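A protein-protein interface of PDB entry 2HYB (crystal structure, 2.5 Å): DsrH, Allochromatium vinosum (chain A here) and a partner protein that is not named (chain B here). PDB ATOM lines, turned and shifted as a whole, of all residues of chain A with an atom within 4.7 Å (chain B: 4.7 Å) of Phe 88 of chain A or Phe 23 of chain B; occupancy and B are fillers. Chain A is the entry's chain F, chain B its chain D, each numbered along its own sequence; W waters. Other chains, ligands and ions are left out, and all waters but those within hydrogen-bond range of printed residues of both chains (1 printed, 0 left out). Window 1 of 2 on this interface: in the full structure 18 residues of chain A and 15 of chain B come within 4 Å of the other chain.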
ATOM      1  N   LEU A   4      15.584  -4.894  -7.287  1.00  0.00           N
ATOM      2  CA  LEU A   4      16.807  -4.225  -6.873  1.00  0.00           C
ATOM      3  C   LEU A   4      16.364  -2.901  -6.270  1.00  0.00           C
ATOM      4  O   LEU A   4      15.855  -2.039  -6.983  1.00  0.00           O
ATOM      5  CB  LEU A   4      17.744  -3.958  -8.050  1.00  0.00           C
ATOM      6  CG  LEU A   4      18.842  -2.939  -7.709  1.00  0.00           C
ATOM      7  CD1 LEU A   4      19.784  -3.503  -6.646  1.00  0.00           C
ATOM      8  CD2 LEU A   4      19.595  -2.558  -8.974  1.00  0.00           C
ATOM      9  N   LEU A  31      21.011  -1.559  -3.117  1.00  0.00           N
ATOM     10  CA  LEU A  31      22.188  -0.787  -3.519  1.00  0.00           C
ATOM     11  C   LEU A  31      22.224   0.565  -2.840  1.00  0.00           C
ATOM     12  O   LEU A  31      21.336   1.389  -3.030  1.00  0.00           O
ATOM     13  CB  LEU A  31      22.214  -0.577  -5.039  1.00  0.00           C
ATOM     14  CG  LEU A  31      23.280   0.396  -5.572  1.00  0.00           C
ATOM     15  CD1 LEU A  31      24.665  -0.092  -5.155  1.00  0.00           C
ATOM     16  CD2 LEU A  31      23.182   0.511  -7.097  1.00  0.00           C
ATOM     17  N   PHE A  33      23.834   4.082  -2.692  1.00  0.00           N
ATOM     18  CA  PHE A  33      24.688   4.982  -3.468  1.00  0.00           C
ATOM     19  C   PHE A  33      24.442   6.432  -3.111  1.00  0.00           C
ATOM     20  O   PHE A  33      23.551   6.737  -2.312  1.00  0.00           O
ATOM     21  CB  PHE A  33      24.581   4.751  -4.988  1.00  0.00           C
ATOM     22  CG  PHE A  33      23.300   5.228  -5.617  1.00  0.00           C
ATOM     23  CD1 PHE A  33      22.075   4.676  -5.255  1.00  0.00           C
ATOM     24  CD2 PHE A  33      23.330   6.186  -6.636  1.00  0.00           C
ATOM     25  CE1 PHE A  33      20.898   5.066  -5.899  1.00  0.00           C
ATOM     26  CE2 PHE A  33      22.163   6.581  -7.284  1.00  0.00           C
ATOM     27  CZ  PHE A  33      20.944   6.019  -6.915  1.00  0.00           C
ATOM     28  N   LEU A  62      27.943   1.538  -3.805  1.00  0.00           N
ATOM     29  CA  LEU A  62      28.642   2.078  -4.967  1.00  0.00           C
ATOM     30  C   LEU A  62      30.005   2.640  -4.562  1.00  0.00           C
ATOM     31  O   LEU A  62      30.104   3.635  -3.836  1.00  0.00           O
ATOM     32  CB  LEU A  62      27.787   3.166  -5.611  1.00  0.00           C
ATOM     33  CG  LEU A  62      28.164   3.629  -7.010  1.00  0.00           C
ATOM     34  CD1 LEU A  62      28.045   2.465  -7.996  1.00  0.00           C
ATOM     35  CD2 LEU A  62      27.246   4.779  -7.421  1.00  0.00           C
ATOM     36  N   VAL A  83      30.594  -2.125  -5.614  1.00  0.00           N
ATOM     37  CA  VAL A  83      30.460  -2.158  -7.072  1.00  0.00           C
ATOM     38  C   VAL A  83      30.655  -0.766  -7.656  1.00  0.00           C
ATOM     39  O   VAL A  83      30.524   0.232  -6.950  1.00  0.00           O
ATOM     40  CB  VAL A  83      29.057  -2.634  -7.506  1.00  0.00           C
ATOM     41  CG1 VAL A  83      28.761  -3.998  -6.925  1.00  0.00           C
ATOM     42  CG2 VAL A  83      28.014  -1.635  -7.068  1.00  0.00           C
ATOM     43  N   ASP A  84      30.974  -0.704  -8.941  1.00  0.00           N
ATOM     44  CA  ASP A  84      31.144   0.574  -9.613  1.00  0.00           C
ATOM     45  C   ASP A  84      29.928   0.728 -10.520  1.00  0.00           C
ATOM     46  O   ASP A  84      29.037  -0.120 -10.507  1.00  0.00           O
ATOM     47  CB  ASP A  84      32.412   0.572 -10.452  1.00  0.00           C
ATOM     48  CG  ASP A  84      32.446  -0.570 -11.441  1.00  0.00           C
ATOM     49  OD1 ASP A  84      31.380  -1.153 -11.727  1.00  0.00           O
ATOM     50  OD2 ASP A  84      33.543  -0.886 -11.938  1.00  0.00           O
ATOM     51  N   TYR A  85      29.884   1.795 -11.311  1.00  0.00           N
ATOM     52  CA  TYR A  85      28.749   1.993 -12.193  1.00  0.00           C
ATOM     53  C   TYR A  85      28.504   0.813 -13.132  1.00  0.00           C
ATOM     54  O   TYR A  85      27.358   0.435 -13.363  1.00  0.00           O
ATOM     55  CB  TYR A  85      28.908   3.290 -12.983  1.00  0.00           C
ATOM     56  CG  TYR A  85      28.700   4.535 -12.138  1.00  0.00           C
ATOM     57  CD1 TYR A  85      29.783   5.292 -11.693  1.00  0.00           C
ATOM     58  CD2 TYR A  85      27.418   4.957 -11.786  1.00  0.00           C
ATOM     59  CE1 TYR A  85      29.591   6.437 -10.926  1.00  0.00           C
ATOM     60  CE2 TYR A  85      27.221   6.094 -11.018  1.00  0.00           C
ATOM     61  CZ  TYR A  85      28.310   6.831 -10.594  1.00  0.00           C
ATOM     62  OH  TYR A  85      28.119   7.977  -9.868  1.00  0.00           O
ATOM     63  N   ALA A  86      29.566   0.229 -13.679  1.00  0.00           N
ATOM     64  CA  ALA A  86      29.408  -0.930 -14.555  1.00  0.00           C
ATOM     65  C   ALA A  86      28.731  -2.051 -13.764  1.00  0.00           C
ATOM     66  O   ALA A  86      28.038  -2.900 -14.329  1.00  0.00           O
ATOM     67  CB  ALA A  86      30.751  -1.394 -15.043  1.00  0.00           C
ATOM     68  N   GLY A  87      28.947  -2.045 -12.450  1.00  0.00           N
ATOM     69  CA  GLY A  87      28.359  -3.053 -11.584  1.00  0.00           C
ATOM     70  C   GLY A  87      26.922  -2.681 -11.287  1.00  0.00           C
ATOM     71  O   GLY A  87      26.042  -3.532 -11.176  1.00  0.00           O
ATOM     72  N   PHE A  88      26.698  -1.382 -11.145  1.00  0.00           N
ATOM     73  CA  PHE A  88      25.376  -0.853 -10.880  1.00  0.00           C
ATOM     74  C   PHE A  88      24.491  -1.373 -12.011  1.00  0.00           C
ATOM     75  O   PHE A  88      23.447  -1.992 -11.782  1.00  0.00           O
ATOM     76  CB  PHE A  88      25.452   0.674 -10.893  1.00  0.00           C
ATOM     77  CG  PHE A  88      24.181   1.365 -10.486  1.00  0.00           C
ATOM     78  CD1 PHE A  88      24.217   2.685 -10.045  1.00  0.00           C
ATOM     79  CD2 PHE A  88      22.952   0.720 -10.556  1.00  0.00           C
ATOM     80  CE1 PHE A  88      23.061   3.350  -9.682  1.00  0.00           C
ATOM     81  CE2 PHE A  88      21.788   1.378 -10.195  1.00  0.00           C
ATOM     82  CZ  PHE A  88      21.840   2.693  -9.758  1.00  0.00           C
ATOM     83  N   VAL A  89      24.944  -1.132 -13.235  1.00  0.00           N
ATOM     84  CA  VAL A  89      24.233  -1.550 -14.430  1.00  0.00           C
ATOM     85  C   VAL A  89      23.868  -3.025 -14.326  1.00  0.00           C
ATOM     86  O   VAL A  89      22.694  -3.383 -14.410  1.00  0.00           O
ATOM     87  CB  VAL A  89      25.106  -1.297 -15.689  1.00  0.00           C
ATOM     88  CG1 VAL A  89      24.431  -1.864 -16.942  1.00  0.00           C
ATOM     89  CG2 VAL A  89      25.346   0.201 -15.852  1.00  0.00           C
ATOM     90  N   ASP A  90      24.866  -3.880 -14.126  1.00  0.00           N
ATOM     91  CA  ASP A  90      24.610  -5.317 -14.012  1.00  0.00           C
ATOM     92  C   ASP A  90      23.529  -5.669 -12.987  1.00  0.00           C
ATOM     93  O   ASP A  90      22.719  -6.563 -13.225  1.00  0.00           O
ATOM     94  CB  ASP A  90      25.895  -6.076 -13.669  1.00  0.00           C
ATOM     95  CG  ASP A  90      26.818  -6.223 -14.859  1.00  0.00           C
ATOM     96  OD1 ASP A  90      26.328  -6.616 -15.942  1.00  0.00           O
ATOM     97  OD2 ASP A  90      28.030  -5.951 -14.707  1.00  0.00           O
ATOM     98  N   LEU A  91      23.518  -4.975 -11.849  1.00  0.00           N
ATOM     99  CA  LEU A  91      22.519  -5.238 -10.825  1.00  0.00           C
ATOM    100  C   LEU A  91      21.128  -4.968 -11.359  1.00  0.00           C
ATOM    101  O   LEU A  91      20.187  -5.694 -11.038  1.00  0.00           O
ATOM    102  CB  LEU A  91      22.750  -4.366  -9.601  1.00  0.00           C
ATOM    103  CG  LEU A  91      23.843  -4.784  -8.623  1.00  0.00           C
ATOM    104  CD1 LEU A  91      23.858  -3.814  -7.442  1.00  0.00           C
ATOM    105  CD2 LEU A  91      23.591  -6.203  -8.142  1.00  0.00           C
ATOM    106  N   THR A  92      20.990  -3.922 -12.172  1.00  0.00           N
ATOM    107  CA  THR A  92      19.678  -3.587 -12.715  1.00  0.00           C
ATOM    108  C   THR A  92      19.239  -4.556 -13.792  1.00  0.00           C
ATOM    109  O   THR A  92      18.070  -4.584 -14.153  1.00  0.00           O
ATOM    110  CB  THR A  92      19.628  -2.171 -13.313  1.00  0.00           C
ATOM    111  OG1 THR A  92      20.477  -2.102 -14.463  1.00  0.00           O
ATOM    112  CG2 THR A  92      20.077  -1.145 -12.293  1.00  0.00           C
ATOM    113  N   PHE B   3      16.759   0.337 -21.627  1.00  0.00           N
ATOM    114  CA  PHE B   3      16.562   1.134 -20.422  1.00  0.00           C
ATOM    115  C   PHE B   3      15.724   2.381 -20.625  1.00  0.00           C
ATOM    116  O   PHE B   3      15.549   2.867 -21.747  1.00  0.00           O
ATOM    117  CB  PHE B   3      17.910   1.555 -19.843  1.00  0.00           C
ATOM    118  CG  PHE B   3      18.609   0.474 -19.100  1.00  0.00           C
ATOM    119  CD1 PHE B   3      18.177   0.096 -17.835  1.00  0.00           C
ATOM    120  CD2 PHE B   3      19.710  -0.164 -19.653  1.00  0.00           C
ATOM    121  CE1 PHE B   3      18.845  -0.901 -17.125  1.00  0.00           C
ATOM    122  CE2 PHE B   3      20.381  -1.162 -18.948  1.00  0.00           C
ATOM    123  CZ  PHE B   3      19.944  -1.529 -17.682  1.00  0.00           C
ATOM    124  N   LEU B   5      15.490   5.978 -18.338  1.00  0.00           N
ATOM    125  CA  LEU B   5      15.979   6.737 -17.192  1.00  0.00           C
ATOM    126  C   LEU B   5      15.160   7.979 -16.879  1.00  0.00           C
ATOM    127  O   LEU B   5      15.024   8.860 -17.724  1.00  0.00           O
ATOM    128  CB  LEU B   5      17.418   7.181 -17.427  1.00  0.00           C
ATOM    129  CG  LEU B   5      18.466   6.214 -17.980  1.00  0.00           C
ATOM    130  CD1 LEU B   5      19.852   6.863 -17.845  1.00  0.00           C
ATOM    131  CD2 LEU B   5      18.429   4.900 -17.222  1.00  0.00           C
ATOM    132  N   SER B  19      24.558  11.054 -11.332  1.00  0.00           N
ATOM    133  CA  SER B  19      24.445   9.600 -11.167  1.00  0.00           C
ATOM    134  C   SER B  19      23.785   8.958 -12.385  1.00  0.00           C
ATOM    135  O   SER B  19      24.234   7.917 -12.868  1.00  0.00           O
ATOM    136  CB  SER B  19      23.624   9.253  -9.922  1.00  0.00           C
ATOM    137  OG  SER B  19      24.232   9.761  -8.761  1.00  0.00           O
ATOM    138  N   ALA B  20      22.716   9.583 -12.871  1.00  0.00           N
ATOM    139  CA  ALA B  20      21.997   9.073 -14.034  1.00  0.00           C
ATOM    140  C   ALA B  20      22.936   9.035 -15.241  1.00  0.00           C
ATOM    141  O   ALA B  20      22.952   8.068 -16.008  1.00  0.00           O
ATOM    142  CB  ALA B  20      20.784   9.955 -14.331  1.00  0.00           C
ATOM    143  N   TYR B  21      23.718  10.098 -15.399  1.00  0.00           N
ATOM    144  CA  TYR B  21      24.668  10.186 -16.493  1.00  0.00           C
ATOM    145  C   TYR B  21      25.713   9.072 -16.396  1.00  0.00           C
ATOM    146  O   TYR B  21      25.965   8.351 -17.369  1.00  0.00           O
ATOM    147  CB  TYR B  21      25.386  11.538 -16.476  1.00  0.00           C
ATOM    148  CG  TYR B  21      26.529  11.589 -17.466  1.00  0.00           C
ATOM    149  CD1 TYR B  21      26.282  11.699 -18.835  1.00  0.00           C
ATOM    150  CD2 TYR B  21      27.851  11.437 -17.045  1.00  0.00           C
ATOM    151  CE1 TYR B  21      27.327  11.647 -19.767  1.00  0.00           C
ATOM    152  CE2 TYR B  21      28.900  11.383 -17.962  1.00  0.00           C
ATOM    153  CZ  TYR B  21      28.632  11.484 -19.322  1.00  0.00           C
ATOM    154  OH  TYR B  21      29.659  11.386 -20.237  1.00  0.00           O
ATOM    155  N   GLN B  22      26.327   8.935 -15.224  1.00  0.00           N
ATOM    156  CA  GLN B  22      27.339   7.905 -15.064  1.00  0.00           C
ATOM    157  C   GLN B  22      26.712   6.569 -15.394  1.00  0.00           C
ATOM    158  O   GLN B  22      27.330   5.732 -16.054  1.00  0.00           O
ATOM    159  CB  GLN B  22      27.912   7.893 -13.641  1.00  0.00           C
ATOM    160  CG  GLN B  22      28.756   9.122 -13.306  1.00  0.00           C
ATOM    161  CD  GLN B  22      29.896   9.362 -14.303  1.00  0.00           C
ATOM    162  OE1 GLN B  22      30.447  10.461 -14.375  1.00  0.00           O
ATOM    163  NE2 GLN B  22      30.258   8.328 -15.062  1.00  0.00           N
ATOM    164  N   PHE B  23      25.470   6.376 -14.959  1.00  0.00           N
ATOM    165  CA  PHE B  23      24.790   5.123 -15.239  1.00  0.00           C
ATOM    166  C   PHE B  23      24.597   4.957 -16.747  1.00  0.00           C
ATOM    167  O   PHE B  23      24.905   3.906 -17.301  1.00  0.00           O
ATOM    168  CB  PHE B  23      23.434   5.074 -14.527  1.00  0.00           C
ATOM    169  CG  PHE B  23      22.713   3.758 -14.678  1.00  0.00           C
ATOM    170  CD1 PHE B  23      22.898   2.731 -13.756  1.00  0.00           C
ATOM    171  CD2 PHE B  23      21.856   3.543 -15.751  1.00  0.00           C
ATOM    172  CE1 PHE B  23      22.232   1.508 -13.910  1.00  0.00           C
ATOM    173  CE2 PHE B  23      21.195   2.331 -15.904  1.00  0.00           C
ATOM    174  CZ  PHE B  23      21.385   1.316 -14.982  1.00  0.00           C
ATOM    175  N   ALA B  24      24.097   5.990 -17.414  1.00  0.00           N
ATOM    176  CA  ALA B  24      23.871   5.886 -18.855  1.00  0.00           C
ATOM    177  C   ALA B  24      25.157   5.623 -19.649  1.00  0.00           C
ATOM    178  O   ALA B  24      25.144   4.834 -20.595  1.00  0.00           O
ATOM    179  CB  ALA B  24      23.168   7.137 -19.380  1.00  0.00           C
ATOM    180  N   LYS B  25      26.264   6.263 -19.278  1.00  0.00           N
ATOM    181  CA  LYS B  25      27.517   6.035 -20.001  1.00  0.00           C
ATOM    182  C   LYS B  25      27.974   4.582 -19.833  1.00  0.00           C
ATOM    183  O   LYS B  25      28.381   3.926 -20.798  1.00  0.00           O
ATOM    184  CB  LYS B  25      28.613   6.975 -19.498  1.00  0.00           C
ATOM    185  CG  LYS B  25      29.816   7.046 -20.427  1.00  0.00           C
ATOM    186  CD  LYS B  25      30.794   8.134 -20.010  1.00  0.00           C
ATOM    187  CE  LYS B  25      31.721   7.667 -18.901  1.00  0.00           C
ATOM    188  NZ  LYS B  25      32.707   6.644 -19.383  1.00  0.00           N
ATOM    189  N   ALA B  26      27.903   4.087 -18.600  1.00  0.00           N
ATOM    190  CA  ALA B  26      28.303   2.719 -18.296  1.00  0.00           C
ATOM    191  C   ALA B  26      27.406   1.712 -19.014  1.00  0.00           C
ATOM    192  O   ALA B  26      27.891   0.715 -19.551  1.00  0.00           O
ATOM    193  CB  ALA B  26      28.257   2.481 -16.788  1.00  0.00           C
ATOM    194  N   ALA B  27      26.101   1.966 -19.018  1.00  0.00           N
ATOM    195  CA  ALA B  27      25.155   1.079 -19.678  1.00  0.00           C
ATOM    196  C   ALA B  27      25.427   1.056 -21.177  1.00  0.00           C
ATOM    197  O   ALA B  27      25.600  -0.007 -21.767  1.00  0.00           O
ATOM    198  CB  ALA B  27      23.730   1.546 -19.406  1.00  0.00           C
ATOM    199  N   VAL B 126      14.812   2.970 -14.451  1.00  0.00           N
ATOM    200  CA  VAL B 126      15.636   3.446 -13.364  1.00  0.00           C
ATOM    201  C   VAL B 126      15.391   4.919 -13.101  1.00  0.00           C
ATOM    202  O   VAL B 126      15.525   5.745 -14.001  1.00  0.00           O
ATOM    203  CB  VAL B 126      17.109   3.199 -13.680  1.00  0.00           C
ATOM    204  CG1 VAL B 126      17.973   3.579 -12.487  1.00  0.00           C
ATOM    205  CG2 VAL B 126      17.296   1.737 -14.056  1.00  0.00           C
ATOM    206  N   PHE B 128      16.267   8.354 -10.839  1.00  0.00           N
ATOM    207  CA  PHE B 128      17.276   9.071 -10.079  1.00  0.00           C
ATOM    208  C   PHE B 128      16.711  10.387  -9.550  1.00  0.00           C
ATOM    209  O   PHE B 128      16.452  11.315 -10.326  1.00  0.00           O
ATOM    210  CB  PHE B 128      18.465   9.404 -10.970  1.00  0.00           C
ATOM    211  CG  PHE B 128      19.177   8.209 -11.519  1.00  0.00           C
ATOM    212  CD1 PHE B 128      18.777   7.636 -12.722  1.00  0.00           C
ATOM    213  CD2 PHE B 128      20.262   7.659 -10.826  1.00  0.00           C
ATOM    214  CE1 PHE B 128      19.453   6.531 -13.230  1.00  0.00           C
ATOM    215  CE2 PHE B 128      20.936   6.566 -11.315  1.00  0.00           C
ATOM    216  CZ  PHE B 128      20.537   5.992 -12.523  1.00  0.00           C
HETATM  217  O   HOH W   1      26.192   7.965  -7.907  1.00  0.00           O
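The backbone carbonyl oxygen (O) of Val 89 of chain A lies within hydrogen-bond range of the side-chain hydroxyl (OG1) of Thr 92 of chain A, 2.6 Å away.
Tyr 85 of chain A touches Ser 19 of chain B.
CB of Gln 22 of chain B touches CZ of Tyr 85 of chain A, at 3.3 Å.
Tyr 85 of chain A touches Phe 23 of chain B (CD2 to N, 3.98 Å).
Ala 26 of chain B touches Tyr 85 of chain A.
CD2 of Phe 88 of chain A touches CE1 of Phe 23 of chain B, at 3.5 Å.
CA of Val 89 of chain A touches CE1 of Phe 23 of chain B, at 3.7 Å.
CG2 of Val 89 of chain A touches CB of Ala 26 of chain B, at 3.8 Å.
N of Ala 27 of chain B touches CG2 of Val 89 of chain A, 3.7 Å away.
Phe 3 of chain B touches Thr 92 of chain A (CZ to OG1, 3.3 Å).
Phe 23 of chain B touches Thr 92 of chain A.
Printed residues of chain B within 4 Å of Val 89 of chain A: Phe 23 (3.7 Å), Ala 26 (3.8 Å) and Ala 27 (3.7 Å).
Leu 91 of chain A touches none of the printed residues of chain B.
Printed residues of chain A within 4 Å of Ser 19 of chain B: Tyr 85.
Printed residues of chain A within 4 Å of Gln 22 of chain B: Tyr 85 (3.3 Å).
Of the printed residues of chain A, Ala 26 of chain B touches Tyr 85 and Val 89.
The nearest residue of chain B that does not touch Phe 88 of chain A is Phe 128 of chain B (4.2 Å).
The nearest printed residue of chain A that does not touch Phe 23 of chain B is Asp 90 of chain A (6.0 Å).
Of the 14 printed residues of chain A, 4 touch a printed residue of chain B.
Printed residues of chain A that touch a printed residue of chain B: Tyr 85, Phe 88, Val 89 and Thr 92.
Hydrophobic or aromatic side chains of chain A within 4 Å of the printed part of chain B: Tyr 85, Phe 88 and Val 89.
Of the 13 printed residues of chain B, 6 touch a printed residue of chain A.
Hydrophobic or aromatic side chains of chain B within 4 Å of the printed part of chain A: Phe 3, Phe 23 and Ala 26.
Among the printed residues, no Asp or Glu carboxylate lies within 4 Å of a Lys or Arg side-chain nitrogen of the other chain.
Water W1 bridges OH of Tyr 85 of chain A (2.7 Å) and OG of Ser 19 of chain B (2.8 Å).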
